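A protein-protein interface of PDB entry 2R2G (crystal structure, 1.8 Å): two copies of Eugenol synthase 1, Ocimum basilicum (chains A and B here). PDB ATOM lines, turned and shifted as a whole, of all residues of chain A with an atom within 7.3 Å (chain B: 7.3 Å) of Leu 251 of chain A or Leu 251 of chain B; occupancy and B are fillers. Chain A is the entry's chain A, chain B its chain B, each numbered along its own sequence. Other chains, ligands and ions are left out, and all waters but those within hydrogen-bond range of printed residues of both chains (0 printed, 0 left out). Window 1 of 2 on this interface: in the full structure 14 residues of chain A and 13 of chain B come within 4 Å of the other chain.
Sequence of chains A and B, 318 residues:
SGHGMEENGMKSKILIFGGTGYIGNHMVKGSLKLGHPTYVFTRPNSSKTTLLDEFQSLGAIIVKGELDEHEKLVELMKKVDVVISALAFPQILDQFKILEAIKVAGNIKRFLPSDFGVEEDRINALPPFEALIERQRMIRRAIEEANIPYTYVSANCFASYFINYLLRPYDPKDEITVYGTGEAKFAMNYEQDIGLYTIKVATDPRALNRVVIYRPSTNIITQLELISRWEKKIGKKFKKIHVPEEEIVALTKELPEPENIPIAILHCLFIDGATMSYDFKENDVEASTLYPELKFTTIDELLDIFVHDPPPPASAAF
Leu 251 of chain A touches two residues of chain B. Printed residues of chain B within 4 Å of Glu 254 of chain A: Val 243 and Glu 247. Printed residues of chain A within 4 Å of Val 243 of chain B: Glu 254 (3.999 Å). No residue of chain A comes within 4 Å of Ala 250 of chain B. Of chain A, only Leu 251 comes within 4 Å of Leu 251 of chain B. Lys 253 of chain B touches none of the printed residues of chain A. Printed residues of chain A within 4 Å of Glu 254 of chain B: Val 243 and Glu 247. The nearest printed residue of chain B that does not touch Leu 251 of chain A is Val 243 of chain B (5.6 Å). The nearest residue of chain A that does not touch Leu 251 of chain B is Glu 247 of chain A (4.3 Å). The nearest printed residue of chain A that does not touch Glu 247 of chain B is Ala 250 of chain A (5.3 Å).
Among the printed residues, merely in contact across the chains: Glu 247 of chain A with Glu 254 of chain B, Glu 254 of chain A with Glu 247 of chain B, Leu 251 of chain A with Leu 251 of chain B, Val 243 of chain A with Glu 254 of chain B, Leu 251 of chain A with Glu 247 of chain B and Glu 254 of chain A with Val 243 of chain B.
The side-chain carboxylate (OE2) of Glu 247 of chain A lies close to the side-chain carboxylate (OE2) of Glu 247 of chain B (2.4 Å).
Val 243 of chain A touches Glu 254 of chain B, and with the chains exchanged Glu 254 of chain A touches Val 243 of chain B. Glu 247 of chain A touches its own counterpart, Glu 247 of chain B. Glu 247 of chain A touches Glu 254 of chain B, and with the chains exchanged Glu 254 of chain A touches Glu 247 of chain B. Leu 251 of chain A touches Glu 247 of chain B, but with the chains exchanged Glu 247 of chain A does not touch Leu 251 of chain B (4.3 Å). 19 positions are printed for both chains. Of the 7 pairs that touch across the chains among the printed residues, 6 have their exchanged pair printed and touching as well.
Hydrophobic or aromatic side chains of chain A that line the printed part of chain B: Val 243 and Leu 251. Among the printed residues, no Asp or Glu carboxylate lies within 4 Å of a Lys or Arg side-chain nitrogen of the other chain.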
ATOM      1  N   PRO A 128      24.163 -16.900 -24.878  1.00  0.00           N
ATOM      2  CA  PRO A 128      23.071 -16.008 -24.474  1.00  0.00           C
ATOM      3  C   PRO A 128      23.522 -14.766 -23.706  1.00  0.00           C
ATOM      4  O   PRO A 128      23.015 -13.667 -23.940  1.00  0.00           O
ATOM      5  CB  PRO A 128      22.173 -16.921 -23.640  1.00  0.00           C
ATOM      6  CG  PRO A 128      22.376 -18.257 -24.293  1.00  0.00           C
ATOM      7  CD  PRO A 128      23.874 -18.292 -24.495  1.00  0.00           C
ATOM      8  N   VAL A 243      21.685 -28.675  -9.497  1.00  0.00           N
ATOM      9  CA  VAL A 243      21.332 -28.661 -10.912  1.00  0.00           C
ATOM     10  C   VAL A 243      22.671 -28.787 -11.625  1.00  0.00           C
ATOM     11  O   VAL A 243      23.445 -27.831 -11.680  1.00  0.00           O
ATOM     12  CB  VAL A 243      20.664 -27.338 -11.326  1.00  0.00           C
ATOM     13  CG1 VAL A 243      20.284 -27.390 -12.797  1.00  0.00           C
ATOM     14  CG2 VAL A 243      19.441 -27.086 -10.470  1.00  0.00           C
ATOM     15  N   PRO A 244      22.969 -29.978 -12.167  1.00  0.00           N
ATOM     16  CA  PRO A 244      24.223 -30.249 -12.877  1.00  0.00           C
ATOM     17  C   PRO A 244      24.606 -29.188 -13.897  1.00  0.00           C
ATOM     18  O   PRO A 244      23.748 -28.633 -14.581  1.00  0.00           O
ATOM     19  CB  PRO A 244      23.960 -31.605 -13.524  1.00  0.00           C
ATOM     20  CG  PRO A 244      23.062 -32.270 -12.520  1.00  0.00           C
ATOM     21  CD  PRO A 244      22.091 -31.162 -12.196  1.00  0.00           C
ATOM     22  N   GLU A 245      25.903 -28.910 -13.990  1.00  0.00           N
ATOM     23  CA  GLU A 245      26.405 -27.916 -14.931  1.00  0.00           C
ATOM     24  C   GLU A 245      26.007 -28.253 -16.362  1.00  0.00           C
ATOM     25  O   GLU A 245      25.481 -27.404 -17.081  1.00  0.00           O
ATOM     26  CB  GLU A 245      27.928 -27.815 -14.847  1.00  0.00           C
ATOM     27  CG  GLU A 245      28.526 -26.904 -15.913  1.00  0.00           C
ATOM     28  CD  GLU A 245      30.026 -26.748 -15.786  1.00  0.00           C
ATOM     29  OE1 GLU A 245      30.626 -27.405 -14.905  1.00  0.00           O
ATOM     30  OE2 GLU A 245      30.606 -25.967 -16.571  1.00  0.00           O
ATOM     31  N   GLU A 246      26.263 -29.490 -16.776  1.00  0.00           N
ATOM     32  CA  GLU A 246      25.926 -29.918 -18.128  1.00  0.00           C
ATOM     33  C   GLU A 246      24.445 -29.687 -18.396  1.00  0.00           C
ATOM     34  O   GLU A 246      24.036 -29.432 -19.530  1.00  0.00           O
ATOM     35  CB  GLU A 246      26.273 -31.398 -18.322  1.00  0.00           C
ATOM     36  CG  GLU A 246      27.761 -31.662 -18.532  1.00  0.00           C
ATOM     37  CD  GLU A 246      28.251 -31.224 -19.907  1.00  0.00           C
ATOM     38  OE1 GLU A 246      28.112 -30.029 -20.249  1.00  0.00           O
ATOM     39  OE2 GLU A 246      28.780 -32.082 -20.648  1.00  0.00           O
ATOM     40  N   GLU A 247      23.645 -29.764 -17.341  1.00  0.00           N
ATOM     41  CA  GLU A 247      22.214 -29.549 -17.464  1.00  0.00           C
ATOM     42  C   GLU A 247      21.940 -28.082 -17.791  1.00  0.00           C
ATOM     43  O   GLU A 247      21.148 -27.764 -18.685  1.00  0.00           O
ATOM     44  CB  GLU A 247      21.511 -29.930 -16.160  1.00  0.00           C
ATOM     45  CG  GLU A 247      20.018 -29.765 -16.235  1.00  0.00           C
ATOM     46  CD  GLU A 247      19.452 -30.463 -17.444  1.00  0.00           C
ATOM     47  OE1 GLU A 247      19.489 -31.711 -17.479  1.00  0.00           O
ATOM     48  OE2 GLU A 247      18.988 -29.763 -18.368  1.00  0.00           O
ATOM     49  N   ILE A 248      22.602 -27.193 -17.058  1.00  0.00           N
ATOM     50  CA  ILE A 248      22.455 -25.753 -17.253  1.00  0.00           C
ATOM     51  C   ILE A 248      22.877 -25.357 -18.667  1.00  0.00           C
ATOM     52  O   ILE A 248      22.178 -24.608 -19.352  1.00  0.00           O
ATOM     53  CB  ILE A 248      23.321 -24.971 -16.232  1.00  0.00           C
ATOM     54  CG1 ILE A 248      22.756 -25.161 -14.821  1.00  0.00           C
ATOM     55  CG2 ILE A 248      23.385 -23.494 -16.610  1.00  0.00           C
ATOM     56  CD1 ILE A 248      21.355 -24.612 -14.644  1.00  0.00           C
ATOM     57  N   VAL A 249      24.027 -25.865 -19.093  1.00  0.00           N
ATOM     58  CA  VAL A 249      24.556 -25.569 -20.419  1.00  0.00           C
ATOM     59  C   VAL A 249      23.576 -25.992 -21.513  1.00  0.00           C
ATOM     60  O   VAL A 249      23.284 -25.222 -22.429  1.00  0.00           O
ATOM     61  CB  VAL A 249      25.906 -26.288 -20.643  1.00  0.00           C
ATOM     62  CG1 VAL A 249      26.372 -26.093 -22.083  1.00  0.00           C
ATOM     63  CG2 VAL A 249      26.947 -25.742 -19.673  1.00  0.00           C
ATOM     64  N   ALA A 250      23.066 -27.213 -21.411  1.00  0.00           N
ATOM     65  CA  ALA A 250      22.124 -27.728 -22.398  1.00  0.00           C
ATOM     66  C   ALA A 250      20.908 -26.817 -22.553  1.00  0.00           C
ATOM     67  O   ALA A 250      20.452 -26.564 -23.669  1.00  0.00           O
ATOM     68  CB  ALA A 250      21.675 -29.131 -22.001  1.00  0.00           C
ATOM     69  N   LEU A 251      20.390 -26.325 -21.432  1.00  0.00           N
ATOM     70  CA  LEU A 251      19.215 -25.452 -21.440  1.00  0.00           C
ATOM     71  C   LEU A 251      19.437 -24.143 -22.190  1.00  0.00           C
ATOM     72  O   LEU A 251      18.537 -23.652 -22.871  1.00  0.00           O
ATOM     73  CB  LEU A 251      18.778 -25.148 -20.004  1.00  0.00           C
ATOM     74  CG  LEU A 251      18.359 -26.345 -19.147  1.00  0.00           C
ATOM     75  CD1 LEU A 251      18.089 -25.887 -17.724  1.00  0.00           C
ATOM     76  CD2 LEU A 251      17.124 -26.996 -19.738  1.00  0.00           C
ATOM     77  N   THR A 252      20.632 -23.574 -22.064  1.00  0.00           N
ATOM     78  CA  THR A 252      20.937 -22.319 -22.740  1.00  0.00           C
ATOM     79  C   THR A 252      20.856 -22.476 -24.258  1.00  0.00           C
ATOM     80  O   THR A 252      20.642 -21.503 -24.980  1.00  0.00           O
ATOM     81  CB  THR A 252      22.352 -21.817 -22.390  1.00  0.00           C
ATOM     82  OG1 THR A 252      23.326 -22.729 -22.916  1.00  0.00           O
ATOM     83  CG2 THR A 252      22.527 -21.717 -20.880  1.00  0.00           C
ATOM     84  N   LYS A 253      21.026 -23.702 -24.738  1.00  0.00           N
ATOM     85  CA  LYS A 253      20.985 -23.969 -26.174  1.00  0.00           C
ATOM     86  C   LYS A 253      19.594 -24.318 -26.693  1.00  0.00           C
ATOM     87  O   LYS A 253      19.273 -24.052 -27.853  1.00  0.00           O
ATOM     88  CB  LYS A 253      21.947 -25.108 -26.520  1.00  0.00           C
ATOM     89  CG  LYS A 253      23.388 -24.849 -26.122  1.00  0.00           C
ATOM     90  CD  LYS A 253      24.256 -26.073 -26.356  1.00  0.00           C
ATOM     91  CE  LYS A 253      25.688 -25.820 -25.909  1.00  0.00           C
ATOM     92  NZ  LYS A 253      26.530 -27.042 -26.022  1.00  0.00           N
ATOM     93  N   GLU A 254      18.768 -24.909 -25.838  1.00  0.00           N
ATOM     94  CA  GLU A 254      17.423 -25.309 -26.248  1.00  0.00           C
ATOM     95  C   GLU A 254      16.296 -24.342 -25.881  1.00  0.00           C
ATOM     96  O   GLU A 254      15.350 -24.172 -26.653  1.00  0.00           O
ATOM     97  CB  GLU A 254      17.122 -26.710 -25.705  1.00  0.00           C
ATOM     98  CG  GLU A 254      17.720 -26.982 -24.337  1.00  0.00           C
ATOM     99  CD  GLU A 254      17.685 -28.452 -23.958  1.00  0.00           C
ATOM    100  OE1 GLU A 254      18.096 -29.291 -24.787  1.00  0.00           O
ATOM    101  OE2 GLU A 254      17.256 -28.766 -22.828  1.00  0.00           O
ATOM    102  N   LEU A 255      16.388 -23.710 -24.716  1.00  0.00           N
ATOM    103  CA  LEU A 255      15.351 -22.774 -24.294  1.00  0.00           C
ATOM    104  C   LEU A 255      15.353 -21.531 -25.170  1.00  0.00           C
ATOM    105  O   LEU A 255      16.394 -21.125 -25.695  1.00  0.00           O
ATOM    106  CB  LEU A 255      15.547 -22.365 -22.830  1.00  0.00           C
ATOM    107  CG  LEU A 255      15.389 -23.448 -21.758  1.00  0.00           C
ATOM    108  CD1 LEU A 255      15.636 -22.841 -20.384  1.00  0.00           C
ATOM    109  CD2 LEU A 255      13.994 -24.052 -21.828  1.00  0.00           C
ATOM    110  N   PRO A 256      14.180 -20.911 -25.352  1.00  0.00           N
ATOM    111  CA  PRO A 256      14.078 -19.704 -26.176  1.00  0.00           C
ATOM    112  C   PRO A 256      14.593 -18.491 -25.411  1.00  0.00           C
ATOM    113  O   PRO A 256      14.952 -18.588 -24.239  1.00  0.00           O
ATOM    114  CB  PRO A 256      12.576 -19.590 -26.451  1.00  0.00           C
ATOM    115  CG  PRO A 256      12.038 -20.977 -26.179  1.00  0.00           C
ATOM    116  CD  PRO A 256      12.842 -21.408 -24.991  1.00  0.00           C
ATOM    117  N   GLU A 259      14.282 -16.535 -21.916  1.00  0.00           N
ATOM    118  CA  GLU A 259      14.373 -17.584 -20.903  1.00  0.00           C
ATOM    119  C   GLU A 259      15.791 -18.118 -20.678  1.00  0.00           C
ATOM    120  O   GLU A 259      16.186 -18.381 -19.542  1.00  0.00           O
ATOM    121  CB  GLU A 259      13.458 -18.763 -21.260  1.00  0.00           C
ATOM    122  CG  GLU A 259      11.971 -18.559 -20.970  1.00  0.00           C
ATOM    123  CD  GLU A 259      11.319 -17.529 -21.871  1.00  0.00           C
ATOM    124  OE1 GLU A 259      11.926 -17.161 -22.898  1.00  0.00           O
ATOM    125  OE2 GLU A 259      10.188 -17.096 -21.555  1.00  0.00           O
ATOM    126  N   ASN A 260      16.564 -18.272 -21.748  1.00  0.00           N
ATOM    127  CA  ASN A 260      17.912 -18.811 -21.608  1.00  0.00           C
ATOM    128  C   ASN A 260      18.965 -17.845 -21.071  1.00  0.00           C
ATOM    129  O   ASN A 260      20.042 -18.275 -20.661  1.00  0.00           O
ATOM    130  CB  ASN A 260      18.386 -19.420 -22.936  1.00  0.00           C
ATOM    131  CG  ASN A 260      18.593 -18.385 -24.025  1.00  0.00           C
ATOM    132  OD1 ASN A 260      18.345 -17.195 -23.834  1.00  0.00           O
ATOM    133  ND2 ASN A 260      19.051 -18.842 -25.187  1.00  0.00           N
ATOM    134  N   ILE A 263      19.638 -18.344 -17.238  1.00  0.00           N
ATOM    135  CA  ILE A 263      20.328 -19.617 -17.093  1.00  0.00           C
ATOM    136  C   ILE A 263      21.821 -19.454 -17.388  1.00  0.00           C
ATOM    137  O   ILE A 263      22.671 -19.910 -16.619  1.00  0.00           O
ATOM    138  CB  ILE A 263      19.714 -20.684 -18.044  1.00  0.00           C
ATOM    139  CG1 ILE A 263      18.251 -20.939 -17.659  1.00  0.00           C
ATOM    140  CG2 ILE A 263      20.508 -21.985 -17.972  1.00  0.00           C
ATOM    141  CD1 ILE A 263      18.068 -21.497 -16.254  1.00  0.00           C
ATOM    142  N   ALA A 264      22.135 -18.786 -18.495  1.00  0.00           N
ATOM    143  CA  ALA A 264      23.527 -18.567 -18.884  1.00  0.00           C
ATOM    144  C   ALA A 264      24.265 -17.722 -17.847  1.00  0.00           C
ATOM    145  O   ALA A 264      25.457 -17.932 -17.595  1.00  0.00           O
ATOM    146  CB  ALA A 264      23.589 -17.890 -20.261  1.00  0.00           C
ATOM    147  N   PRO B 128       4.464 -29.857  -9.319  1.00  0.00           N
ATOM    148  CA  PRO B 128       4.399 -28.391  -9.339  1.00  0.00           C
ATOM    149  C   PRO B 128       3.040 -27.839  -9.764  1.00  0.00           C
ATOM    150  O   PRO B 128       2.557 -26.855  -9.200  1.00  0.00           O
ATOM    151  CB  PRO B 128       5.515 -28.011 -10.311  1.00  0.00           C
ATOM    152  CG  PRO B 128       6.526 -29.102 -10.086  1.00  0.00           C
ATOM    153  CD  PRO B 128       5.647 -30.340 -10.053  1.00  0.00           C
ATOM    154  N   VAL B 243      13.002 -30.000 -26.932  1.00  0.00           N
ATOM    155  CA  VAL B 243      13.392 -30.142 -25.539  1.00  0.00           C
ATOM    156  C   VAL B 243      12.808 -31.490 -25.138  1.00  0.00           C
ATOM    157  O   VAL B 243      11.590 -31.649 -25.054  1.00  0.00           O
ATOM    158  CB  VAL B 243      12.791 -29.035 -24.648  1.00  0.00           C
ATOM    159  CG1 VAL B 243      13.298 -29.185 -23.216  1.00  0.00           C
ATOM    160  CG2 VAL B 243      13.160 -27.670 -25.198  1.00  0.00           C
ATOM    161  N   PRO B 244      13.672 -32.493 -24.918  1.00  0.00           N
ATOM    162  CA  PRO B 244      13.226 -33.834 -24.530  1.00  0.00           C
ATOM    163  C   PRO B 244      12.311 -33.823 -23.314  1.00  0.00           C
ATOM    164  O   PRO B 244      12.484 -33.012 -22.407  1.00  0.00           O
ATOM    165  CB  PRO B 244      14.539 -34.564 -24.257  1.00  0.00           C
ATOM    166  CG  PRO B 244      15.475 -33.921 -25.228  1.00  0.00           C
ATOM    167  CD  PRO B 244      15.135 -32.455 -25.075  1.00  0.00           C
ATOM    168  N   GLU B 245      11.337 -34.726 -23.304  1.00  0.00           N
ATOM    169  CA  GLU B 245      10.400 -34.819 -22.191  1.00  0.00           C
ATOM    170  C   GLU B 245      11.137 -35.086 -20.884  1.00  0.00           C
ATOM    171  O   GLU B 245      10.923 -34.390 -19.889  1.00  0.00           O
ATOM    172  CB  GLU B 245       9.383 -35.936 -22.435  1.00  0.00           C
ATOM    173  CG  GLU B 245       8.501 -36.214 -21.226  1.00  0.00           C
ATOM    174  CD  GLU B 245       7.474 -37.295 -21.477  1.00  0.00           C
ATOM    175  OE1 GLU B 245       7.561 -37.978 -22.521  1.00  0.00           O
ATOM    176  OE2 GLU B 245       6.579 -37.465 -20.621  1.00  0.00           O
ATOM    177  N   GLU B 246      12.007 -36.091 -20.886  1.00  0.00           N
ATOM    178  CA  GLU B 246      12.766 -36.436 -19.689  1.00  0.00           C
ATOM    179  C   GLU B 246      13.495 -35.207 -19.167  1.00  0.00           C
ATOM    180  O   GLU B 246      13.713 -35.060 -17.965  1.00  0.00           O
ATOM    181  CB  GLU B 246      13.765 -37.553 -19.995  1.00  0.00           C
ATOM    182  CG  GLU B 246      13.138 -38.939 -20.076  1.00  0.00           C
ATOM    183  CD  GLU B 246      12.711 -39.475 -18.715  1.00  0.00           C
ATOM    184  OE1 GLU B 246      11.870 -38.833 -18.045  1.00  0.00           O
ATOM    185  OE2 GLU B 246      13.220 -40.546 -18.314  1.00  0.00           O
ATOM    186  N   GLU B 247      13.866 -34.320 -20.083  1.00  0.00           N
ATOM    187  CA  GLU B 247      14.552 -33.094 -19.719  1.00  0.00           C
ATOM    188  C   GLU B 247      13.597 -32.181 -18.942  1.00  0.00           C
ATOM    189  O   GLU B 247      13.951 -31.628 -17.900  1.00  0.00           O
ATOM    190  CB  GLU B 247      15.050 -32.386 -20.982  1.00  0.00           C
ATOM    191  CG  GLU B 247      15.774 -31.093 -20.704  1.00  0.00           C
ATOM    192  CD  GLU B 247      16.846 -31.272 -19.659  1.00  0.00           C
ATOM    193  OE1 GLU B 247      17.795 -32.049 -19.908  1.00  0.00           O
ATOM    194  OE2 GLU B 247      16.731 -30.646 -18.584  1.00  0.00           O
ATOM    195  N   ILE B 248      12.382 -32.036 -19.461  1.00  0.00           N
ATOM    196  CA  ILE B 248      11.365 -31.200 -18.834  1.00  0.00           C
ATOM    197  C   ILE B 248      10.996 -31.724 -17.442  1.00  0.00           C
ATOM    198  O   ILE B 248      10.878 -30.953 -16.490  1.00  0.00           O
ATOM    199  CB  ILE B 248      10.094 -31.149 -19.716  1.00  0.00           C
ATOM    200  CG1 ILE B 248      10.412 -30.430 -21.033  1.00  0.00           C
ATOM    201  CG2 ILE B 248       8.955 -30.472 -18.975  1.00  0.00           C
ATOM    202  CD1 ILE B 248      10.886 -29.003 -20.858  1.00  0.00           C
ATOM    203  N   VAL B 249      10.817 -33.036 -17.338  1.00  0.00           N
ATOM    204  CA  VAL B 249      10.470 -33.676 -16.073  1.00  0.00           C
ATOM    205  C   VAL B 249      11.553 -33.452 -15.015  1.00  0.00           C
ATOM    206  O   VAL B 249      11.254 -33.102 -13.874  1.00  0.00           O
ATOM    207  CB  VAL B 249      10.261 -35.200 -16.270  1.00  0.00           C
ATOM    208  CG1 VAL B 249      10.045 -35.885 -14.921  1.00  0.00           C
ATOM    209  CG2 VAL B 249       9.065 -35.441 -17.184  1.00  0.00           C
ATOM    210  N   ALA B 250      12.811 -33.651 -15.394  1.00  0.00           N
ATOM    211  CA  ALA B 250      13.914 -33.461 -14.459  1.00  0.00           C
ATOM    212  C   ALA B 250      13.925 -32.045 -13.889  1.00  0.00           C
ATOM    213  O   ALA B 250      14.128 -31.853 -12.691  1.00  0.00           O
ATOM    214  CB  ALA B 250      15.243 -33.762 -15.145  1.00  0.00           C
ATOM    215  N   LEU B 251      13.698 -31.057 -14.746  1.00  0.00           N
ATOM    216  CA  LEU B 251      13.693 -29.660 -14.325  1.00  0.00           C
ATOM    217  C   LEU B 251      12.637 -29.351 -13.266  1.00  0.00           C
ATOM    218  O   LEU B 251      12.896 -28.593 -12.331  1.00  0.00           O
ATOM    219  CB  LEU B 251      13.486 -28.747 -15.540  1.00  0.00           C
ATOM    220  CG  LEU B 251      14.618 -28.715 -16.572  1.00  0.00           C
ATOM    221  CD1 LEU B 251      14.194 -27.912 -17.791  1.00  0.00           C
ATOM    222  CD2 LEU B 251      15.860 -28.115 -15.941  1.00  0.00           C
ATOM    223  N   THR B 252      11.447 -29.936 -13.405  1.00  0.00           N
ATOM    224  CA  THR B 252      10.372 -29.697 -12.444  1.00  0.00           C
ATOM    225  C   THR B 252      10.771 -30.167 -11.048  1.00  0.00           C
ATOM    226  O   THR B 252      10.226 -29.700 -10.051  1.00  0.00           O
ATOM    227  CB  THR B 252       9.078 -30.441 -12.831  1.00  0.00           C
ATOM    228  OG1 THR B 252       9.278 -31.858 -12.712  1.00  0.00           O
ATOM    229  CG2 THR B 252       8.689 -30.104 -14.258  1.00  0.00           C
ATOM    230  N   LYS B 253      11.723 -31.091 -10.982  1.00  0.00           N
ATOM    231  CA  LYS B 253      12.161 -31.628  -9.705  1.00  0.00           C
ATOM    232  C   LYS B 253      13.348 -30.898  -9.102  1.00  0.00           C
ATOM    233  O   LYS B 253      13.547 -30.927  -7.880  1.00  0.00           O
ATOM    234  CB  LYS B 253      12.512 -33.118  -9.846  1.00  0.00           C
ATOM    235  CG  LYS B 253      11.373 -33.996 -10.341  1.00  0.00           C
ATOM    236  CD  LYS B 253      11.851 -35.427 -10.568  1.00  0.00           C
ATOM    237  CE  LYS B 253      10.758 -36.270 -11.202  1.00  0.00           C
ATOM    238  NZ  LYS B 253      11.248 -37.631 -11.543  1.00  0.00           N
ATOM    239  N   GLU B 254      14.150 -30.246  -9.942  1.00  0.00           N
ATOM    240  CA  GLU B 254      15.347 -29.547  -9.457  1.00  0.00           C
ATOM    241  C   GLU B 254      15.252 -28.039  -9.324  1.00  0.00           C
ATOM    242  O   GLU B 254      15.846 -27.435  -8.418  1.00  0.00           O
ATOM    243  CB  GLU B 254      16.536 -29.940 -10.306  1.00  0.00           C
ATOM    244  CG  GLU B 254      16.244 -30.103 -11.792  1.00  0.00           C
ATOM    245  CD  GLU B 254      17.387 -30.793 -12.524  1.00  0.00           C
ATOM    246  OE1 GLU B 254      17.789 -31.888 -12.077  1.00  0.00           O
ATOM    247  OE2 GLU B 254      17.881 -30.246 -13.537  1.00  0.00           O
ATOM    248  N   LEU B 255      14.504 -27.411 -10.226  1.00  0.00           N
ATOM    249  CA  LEU B 255      14.325 -25.974 -10.191  1.00  0.00           C
ATOM    250  C   LEU B 255      13.388 -25.617  -9.058  1.00  0.00           C
ATOM    251  O   LEU B 255      12.424 -26.326  -8.794  1.00  0.00           O
ATOM    252  CB  LEU B 255      13.763 -25.453 -11.515  1.00  0.00           C
ATOM    253  CG  LEU B 255      14.653 -25.584 -12.756  1.00  0.00           C
ATOM    254  CD1 LEU B 255      13.992 -24.952 -13.971  1.00  0.00           C
ATOM    255  CD2 LEU B 255      15.979 -24.886 -12.464  1.00  0.00           C
ATOM    256  N   PRO B 256      13.653 -24.503  -8.355  1.00  0.00           N
ATOM    257  CA  PRO B 256      12.793 -24.077  -7.230  1.00  0.00           C
ATOM    258  C   PRO B 256      11.490 -23.472  -7.735  1.00  0.00           C
ATOM    259  O   PRO B 256      11.322 -23.250  -8.929  1.00  0.00           O
ATOM    260  CB  PRO B 256      13.645 -23.003  -6.542  1.00  0.00           C
ATOM    261  CG  PRO B 256      14.339 -22.372  -7.720  1.00  0.00           C
ATOM    262  CD  PRO B 256      14.793 -23.573  -8.517  1.00  0.00           C
ATOM    263  N   GLU B 259       9.617 -20.973 -10.558  1.00  0.00           N
ATOM    264  CA  GLU B 259      10.232 -21.391 -11.808  1.00  0.00           C
ATOM    265  C   GLU B 259       9.779 -22.746 -12.360  1.00  0.00           C
ATOM    266  O   GLU B 259       9.543 -22.886 -13.557  1.00  0.00           O
ATOM    267  CB  GLU B 259      11.762 -21.399 -11.671  1.00  0.00           C
ATOM    268  CG  GLU B 259      12.423 -20.030 -11.522  1.00  0.00           C
ATOM    269  CD  GLU B 259      12.235 -19.404 -10.148  1.00  0.00           C
ATOM    270  OE1 GLU B 259      11.643 -20.054  -9.261  1.00  0.00           O
ATOM    271  OE2 GLU B 259      12.690 -18.253  -9.955  1.00  0.00           O
ATOM    272  N   ASN B 260       9.648 -23.751 -11.500  1.00  0.00           N
ATOM    273  CA  ASN B 260       9.258 -25.080 -11.965  1.00  0.00           C
ATOM    274  C   ASN B 260       7.787 -25.251 -12.341  1.00  0.00           C
ATOM    275  O   ASN B 260       7.421 -26.254 -12.950  1.00  0.00           O
ATOM    276  CB  ASN B 260       9.652 -26.147 -10.932  1.00  0.00           C
ATOM    277  CG  ASN B 260       8.818 -26.083  -9.676  1.00  0.00           C
ATOM    278  OD1 ASN B 260       8.015 -25.172  -9.495  1.00  0.00           O
ATOM    279  ND2 ASN B 260       9.011 -27.052  -8.788  1.00  0.00           N
ATOM    280  N   ILE B 263       7.165 -24.928 -16.260  1.00  0.00           N
ATOM    281  CA  ILE B 263       7.753 -26.117 -16.864  1.00  0.00           C
ATOM    282  C   ILE B 263       6.782 -27.292 -16.740  1.00  0.00           C
ATOM    283  O   ILE B 263       6.539 -28.011 -17.710  1.00  0.00           O
ATOM    284  CB  ILE B 263       9.113 -26.461 -16.189  1.00  0.00           C
ATOM    285  CG1 ILE B 263      10.131 -25.356 -16.484  1.00  0.00           C
ATOM    286  CG2 ILE B 263       9.640 -27.798 -16.696  1.00  0.00           C
ATOM    287  CD1 ILE B 263      10.454 -25.197 -17.964  1.00  0.00           C
ATOM    288  N   ALA B 264       6.219 -27.478 -15.550  1.00  0.00           N
ATOM    289  CA  ALA B 264       5.272 -28.570 -15.328  1.00  0.00           C
ATOM    290  C   ALA B 264       4.021 -28.407 -16.197  1.00  0.00           C
ATOM    291  O   ALA B 264       3.457 -29.390 -16.694  1.00  0.00           O
ATOM    292  CB  ALA B 264       4.881 -28.639 -13.849  1.00  0.00           C
